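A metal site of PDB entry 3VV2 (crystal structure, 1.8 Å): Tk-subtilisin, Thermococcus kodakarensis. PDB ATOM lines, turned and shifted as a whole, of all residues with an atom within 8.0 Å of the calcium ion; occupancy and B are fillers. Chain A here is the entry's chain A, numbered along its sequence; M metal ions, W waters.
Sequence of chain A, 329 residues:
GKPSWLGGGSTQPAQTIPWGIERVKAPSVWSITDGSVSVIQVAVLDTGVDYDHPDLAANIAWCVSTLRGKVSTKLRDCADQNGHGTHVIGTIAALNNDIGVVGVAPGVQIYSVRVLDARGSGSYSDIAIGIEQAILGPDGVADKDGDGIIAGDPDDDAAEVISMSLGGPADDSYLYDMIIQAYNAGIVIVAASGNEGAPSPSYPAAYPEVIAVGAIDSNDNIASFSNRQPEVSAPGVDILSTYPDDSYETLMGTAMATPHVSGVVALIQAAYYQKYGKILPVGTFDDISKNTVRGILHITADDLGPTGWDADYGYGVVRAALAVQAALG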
ATOM      1  N   VAL A  37      16.860  -5.097   1.040  1.00  0.00           N
ATOM      2  CA  VAL A  37      16.196  -4.052   0.342  1.00  0.00           C
ATOM      3  C   VAL A  37      14.873  -3.741   1.083  1.00  0.00           C
ATOM      4  O   VAL A  37      14.050  -4.613   1.255  1.00  0.00           O
ATOM      5  CB  VAL A  37      15.986  -4.497  -1.121  1.00  0.00           C
ATOM      6  CG1 VAL A  37      15.301  -3.444  -1.931  1.00  0.00           C
ATOM      7  CG2 VAL A  37      17.264  -4.838  -1.729  1.00  0.00           C
ATOM      8  N   SER A  38      14.694  -2.503   1.515  1.00  0.00           N
ATOM      9  CA  SER A  38      13.607  -2.165   2.447  1.00  0.00           C
ATOM     10  C   SER A  38      12.143  -2.598   2.083  1.00  0.00           C
ATOM     11  O   SER A  38      11.319  -2.958   2.975  1.00  0.00           O
ATOM     12  CB  SER A  38      13.671  -0.626   2.738  1.00  0.00           C
ATOM     13  OG  SER A  38      12.576  -0.246   3.549  1.00  0.00           O
ATOM     14  N   VAL A  39      11.819  -2.636   0.793  1.00  0.00           N
ATOM     15  CA  VAL A  39      10.455  -3.016   0.429  1.00  0.00           C
ATOM     16  C   VAL A  39      10.212  -4.580   0.622  1.00  0.00           C
ATOM     17  O   VAL A  39       9.054  -5.009   0.669  1.00  0.00           O
ATOM     18  CB  VAL A  39      10.119  -2.583  -1.019  1.00  0.00           C
ATOM     19  CG1 VAL A  39      10.954  -3.356  -2.008  1.00  0.00           C
ATOM     20  CG2 VAL A  39       8.617  -2.836  -1.321  1.00  0.00           C
ATOM     21  N   ILE A  40      11.304  -5.351   0.673  1.00  0.00           N
ATOM     22  CA  ILE A  40      11.232  -6.858   0.704  1.00  0.00           C
ATOM     23  C   ILE A  40      11.064  -7.441   2.115  1.00  0.00           C
ATOM     24  O   ILE A  40      11.884  -7.221   3.013  1.00  0.00           O
ATOM     25  CB  ILE A  40      12.500  -7.495   0.035  1.00  0.00           C
ATOM     26  CG1 ILE A  40      12.734  -6.922  -1.369  1.00  0.00           C
ATOM     27  CG2 ILE A  40      12.465  -9.092   0.052  1.00  0.00           C
ATOM     28  CD1 ILE A  40      11.610  -7.188  -2.370  1.00  0.00           C
ATOM     29  N   GLN A  41       9.957  -8.166   2.326  1.00  0.00           N
ATOM     30  CA  GLN A  41       9.858  -9.008   3.518  1.00  0.00           C
ATOM     31  C   GLN A  41       9.523 -10.467   3.111  1.00  0.00           C
ATOM     32  O   GLN A  41       8.858 -10.681   2.104  1.00  0.00           O
ATOM     33  CB  GLN A  41       8.719  -8.489   4.402  1.00  0.00           C
ATOM     34  CG  GLN A  41       9.062  -7.123   5.049  1.00  0.00           C
ATOM     35  CD  GLN A  41       8.730  -5.985   4.076  1.00  0.00           C
ATOM     36  OE1 GLN A  41       7.848  -6.104   3.205  1.00  0.00           O
ATOM     37  NE2 GLN A  41       9.437  -4.880   4.218  1.00  0.00           N
ATOM     38  N   VAL A  42      10.000 -11.414   3.911  1.00  0.00           N
ATOM     39  CA  VAL A  42       9.596 -12.803   3.745  1.00  0.00           C
ATOM     40  C   VAL A  42       8.810 -13.168   4.974  1.00  0.00           C
ATOM     41  O   VAL A  42       9.320 -13.034   6.103  1.00  0.00           O
ATOM     42  CB  VAL A  42      10.823 -13.757   3.566  1.00  0.00           C
ATOM     43  CG1 VAL A  42      10.312 -15.147   3.422  1.00  0.00           C
ATOM     44  CG2 VAL A  42      11.710 -13.318   2.362  1.00  0.00           C
ATOM     45  N   GLN A 109      14.411  -8.964   5.765  1.00  0.00           N
ATOM     46  CA  GLN A 109      13.429  -8.790   6.803  1.00  0.00           C
ATOM     47  C   GLN A 109      12.473  -9.975   6.823  1.00  0.00           C
ATOM     48  O   GLN A 109      11.897 -10.337   5.826  1.00  0.00           O
ATOM     49  CB  GLN A 109      12.580  -7.541   6.535  1.00  0.00           C
ATOM     50  CG  GLN A 109      13.233  -6.196   6.774  1.00  0.00           C
ATOM     51  CD  GLN A 109      12.434  -5.158   6.005  1.00  0.00           C
ATOM     52  OE1 GLN A 109      11.294  -4.806   6.370  1.00  0.00           O
ATOM     53  NE2 GLN A 109      13.012  -4.698   4.886  1.00  0.00           N
ATOM     54  N   TYR A 111       8.853 -11.716   8.502  1.00  0.00           N
ATOM     55  CA  TYR A 111       7.672 -11.741   9.317  1.00  0.00           C
ATOM     56  C   TYR A 111       7.503 -13.170   9.768  1.00  0.00           C
ATOM     57  O   TYR A 111       7.260 -14.100   8.934  1.00  0.00           O
ATOM     58  CB  TYR A 111       6.446 -11.334   8.480  1.00  0.00           C
ATOM     59  CG  TYR A 111       6.357  -9.901   7.923  1.00  0.00           C
ATOM     60  CD1 TYR A 111       7.164  -8.902   8.375  1.00  0.00           C
ATOM     61  CD2 TYR A 111       5.369  -9.578   6.973  1.00  0.00           C
ATOM     62  CE1 TYR A 111       7.027  -7.605   7.899  1.00  0.00           C
ATOM     63  CE2 TYR A 111       5.242  -8.317   6.477  1.00  0.00           C
ATOM     64  CZ  TYR A 111       6.060  -7.330   6.955  1.00  0.00           C
ATOM     65  OH  TYR A 111       5.907  -6.043   6.488  1.00  0.00           O
ATOM     66  N   ALA A 134       0.055 -12.107   6.303  1.00  0.00           N
ATOM     67  CA  ALA A 134       1.207 -11.830   5.442  1.00  0.00           C
ATOM     68  C   ALA A 134       0.863 -10.790   4.370  1.00  0.00           C
ATOM     69  O   ALA A 134       1.698 -10.009   3.997  1.00  0.00           O
ATOM     70  CB  ALA A 134       1.754 -13.172   4.763  1.00  0.00           C
ATOM     71  N   ILE A 150       0.631  -4.548  -4.442  1.00  0.00           N
ATOM     72  CA  ILE A 150       0.745  -4.926  -3.056  1.00  0.00           C
ATOM     73  C   ILE A 150       2.172  -5.409  -2.752  1.00  0.00           C
ATOM     74  O   ILE A 150       2.919  -4.725  -2.116  1.00  0.00           O
ATOM     75  CB  ILE A 150      -0.345  -5.939  -2.641  1.00  0.00           C
ATOM     76  CG1 ILE A 150      -1.730  -5.336  -2.797  1.00  0.00           C
ATOM     77  CG2 ILE A 150      -0.155  -6.361  -1.199  1.00  0.00           C
ATOM     78  CD1 ILE A 150      -2.759  -6.306  -3.102  1.00  0.00           C
ATOM     79  N   ALA A 151       2.575  -6.553  -3.265  1.00  0.00           N
ATOM     80  CA  ALA A 151       3.934  -6.996  -3.006  1.00  0.00           C
ATOM     81  C   ALA A 151       4.672  -6.036  -3.933  1.00  0.00           C
ATOM     82  O   ALA A 151       4.180  -5.722  -5.044  1.00  0.00           O
ATOM     83  CB  ALA A 151       4.113  -8.475  -3.470  1.00  0.00           C
ATOM     84  N   GLY A 152       5.816  -5.545  -3.464  1.00  0.00           N
ATOM     85  CA  GLY A 152       6.625  -4.582  -4.231  1.00  0.00           C
ATOM     86  C   GLY A 152       6.227  -3.112  -4.214  1.00  0.00           C
ATOM     87  O   GLY A 152       6.954  -2.252  -4.766  1.00  0.00           O
ATOM     88  N   ASP A 153       5.090  -2.791  -3.616  1.00  0.00           N
ATOM     89  CA  ASP A 153       4.724  -1.403  -3.396  1.00  0.00           C
ATOM     90  C   ASP A 153       5.394  -0.867  -2.155  1.00  0.00           C
ATOM     91  O   ASP A 153       5.121  -1.325  -1.061  1.00  0.00           O
ATOM     92  CB  ASP A 153       3.211  -1.256  -3.301  1.00  0.00           C
ATOM     93  CG  ASP A 153       2.758   0.188  -3.312  1.00  0.00           C
ATOM     94  OD1 ASP A 153       1.572   0.433  -3.563  1.00  0.00           O
ATOM     95  OD2 ASP A 153       3.521   1.125  -3.082  1.00  0.00           O
ATOM     96  N   PRO A 154       6.298   0.089  -2.301  1.00  0.00           N
ATOM     97  CA  PRO A 154       6.928   0.568  -1.054  1.00  0.00           C
ATOM     98  C   PRO A 154       6.007   1.264  -0.047  1.00  0.00           C
ATOM     99  O   PRO A 154       6.419   1.393   1.114  1.00  0.00           O
ATOM    100  CB  PRO A 154       8.024   1.520  -1.523  1.00  0.00           C
ATOM    101  CG  PRO A 154       7.618   1.928  -2.960  1.00  0.00           C
ATOM    102  CD  PRO A 154       6.752   0.818  -3.513  1.00  0.00           C
ATOM    103  N   ASP A 155       4.812   1.678  -0.482  1.00  0.00           N
ATOM    104  CA  ASP A 155       3.796   2.343   0.385  1.00  0.00           C
ATOM    105  C   ASP A 155       3.059   1.270   1.218  1.00  0.00           C
ATOM    106  O   ASP A 155       2.501   1.537   2.322  1.00  0.00           O
ATOM    107  CB  ASP A 155       2.777   3.198  -0.412  1.00  0.00           C
ATOM    108  CG  ASP A 155       1.833   3.918   0.498  1.00  0.00           C
ATOM    109  OD1 ASP A 155       2.342   4.607   1.402  1.00  0.00           O
ATOM    110  OD2 ASP A 155       0.595   3.758   0.415  1.00  0.00           O
ATOM    111  N   ASP A 156       3.089   0.044   0.733  1.00  0.00           N
ATOM    112  CA  ASP A 156       2.533  -1.042   1.562  1.00  0.00           C
ATOM    113  C   ASP A 156       3.587  -1.853   2.373  1.00  0.00           C
ATOM    114  O   ASP A 156       4.794  -1.673   2.213  1.00  0.00           O
ATOM    115  CB  ASP A 156       1.674  -1.992   0.733  1.00  0.00           C
ATOM    116  CG  ASP A 156       0.370  -1.340   0.239  1.00  0.00           C
ATOM    117  OD1 ASP A 156      -0.398  -0.847   1.090  1.00  0.00           O
ATOM    118  OD2 ASP A 156       0.115  -1.332  -0.980  1.00  0.00           O
ATOM    119  N   ASP A 157       3.102  -2.732   3.229  1.00  0.00           N
ATOM    120  CA  ASP A 157       3.975  -3.551   4.065  1.00  0.00           C
ATOM    121  C   ASP A 157       3.696  -5.028   3.880  1.00  0.00           C
ATOM    122  O   ASP A 157       3.964  -5.835   4.769  1.00  0.00           O
ATOM    123  CB  ASP A 157       3.822  -3.159   5.538  1.00  0.00           C
ATOM    124  CG  ASP A 157       2.386  -3.223   6.012  1.00  0.00           C
ATOM    125  OD1 ASP A 157       2.130  -2.844   7.176  1.00  0.00           O
ATOM    126  OD2 ASP A 157       1.517  -3.637   5.224  1.00  0.00           O
ATOM    127  N   ALA A 158       3.146  -5.395   2.727  1.00  0.00           N
ATOM    128  CA  ALA A 158       2.857  -6.798   2.451  1.00  0.00           C
ATOM    129  C   ALA A 158       4.178  -7.530   2.285  1.00  0.00           C
ATOM    130  O   ALA A 158       5.137  -6.946   1.820  1.00  0.00           O
ATOM    131  CB  ALA A 158       2.031  -6.928   1.141  1.00  0.00           C
ATOM    132  N   ALA A 159       4.218  -8.817   2.636  1.00  0.00           N
ATOM    133  CA  ALA A 159       5.408  -9.612   2.323  1.00  0.00           C
ATOM    134  C   ALA A 159       5.485  -9.851   0.822  1.00  0.00           C
ATOM    135  O   ALA A 159       4.453  -9.801   0.123  1.00  0.00           O
ATOM    136  CB  ALA A 159       5.332 -11.008   3.086  1.00  0.00           C
ATOM    137  N   GLU A 160       6.692 -10.127   0.341  1.00  0.00           N
ATOM    138  CA  GLU A 160       6.886 -10.545  -1.050  1.00  0.00           C
ATOM    139  C   GLU A 160       6.994 -12.029  -1.247  1.00  0.00           C
ATOM    140  O   GLU A 160       6.930 -12.493  -2.410  1.00  0.00           O
ATOM    141  CB  GLU A 160       8.115  -9.834  -1.662  1.00  0.00           C
ATOM    142  CG  GLU A 160       7.881  -8.309  -2.057  1.00  0.00           C
ATOM    143  CD  GLU A 160       7.524  -7.374  -0.845  1.00  0.00           C
ATOM    144  OE1 GLU A 160       6.777  -6.403  -1.042  1.00  0.00           O
ATOM    145  OE2 GLU A 160       7.963  -7.619   0.295  1.00  0.00           O
ATOM    146  N   VAL A 161       7.231 -12.759  -0.155  1.00  0.00           N
ATOM    147  CA  VAL A 161       7.384 -14.216  -0.230  1.00  0.00           C
ATOM    148  C   VAL A 161       6.577 -14.745   0.925  1.00  0.00           C
ATOM    149  O   VAL A 161       6.623 -14.196   2.017  1.00  0.00           O
ATOM    150  CB  VAL A 161       8.879 -14.666  -0.125  1.00  0.00           C
ATOM    151  CG1 VAL A 161       9.007 -16.183  -0.151  1.00  0.00           C
ATOM    152  CG2 VAL A 161       9.745 -13.976  -1.191  1.00  0.00           C
ATOM    153  N   ILE A 279       9.353  -5.271  -8.709  1.00  0.00           N
ATOM    154  CA  ILE A 279       9.695  -6.669  -8.570  1.00  0.00           C
ATOM    155  C   ILE A 279       9.293  -7.423  -9.822  1.00  0.00           C
ATOM    156  O   ILE A 279       8.565  -6.870 -10.676  1.00  0.00           O
ATOM    157  CB  ILE A 279       9.003  -7.288  -7.303  1.00  0.00           C
ATOM    158  CG1 ILE A 279       7.477  -7.198  -7.396  1.00  0.00           C
ATOM    159  CG2 ILE A 279       9.603  -6.599  -6.058  1.00  0.00           C
ATOM    160  CD1 ILE A 279       6.694  -7.946  -6.258  1.00  0.00           C
HETATM  161 CA    CA M   1       6.953  -5.555   1.064  1.00  0.00          CA
HETATM  162  O   HOH W   1       4.921  -4.148  -0.140  1.00  0.00           O
HETATM  163  O   HOH W   2       6.891  -3.371   2.014  1.00  0.00           O
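The calcium ion is bound by O of Val 39, 2.2 Å away.
The calcium ion is bound by the side-chain carboxylate (OE1) of Glu 160 (2.3 Å).
Water W2 binds the calcium ion (2.4 Å).
OE1 of Gln 41 is bound to the calcium ion (2.4 Å).
O of Ala 158 binds the calcium ion.
The side-chain carboxylate (OE2) of Glu 160 is bound to the calcium ion, 2.4 Å away.
Water W1 binds the calcium ion (2.7 Å).
Four residues have an atom within 4 Å of the calcium ion: Val 39, Gln 41, Ala 158 and Glu 160.
The side-chain carboxylate (OE1) of Glu 160 lies close to the backbone NH (N) of Gly 152 (2.7 Å).
The backbone carbonyl oxygen (O) of Ser 38 lies within hydrogen-bond range of the side-chain amide nitrogen (NE2) of Gln 41.
The side-chain amide nitrogen of Gln 41 sits at hydrogen-bond distance from the side-chain amide oxygen of Gln 109 (2.8 Å).
N of Val 161 lies within hydrogen-bond range of O of Gln 41 (3.5 Å).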
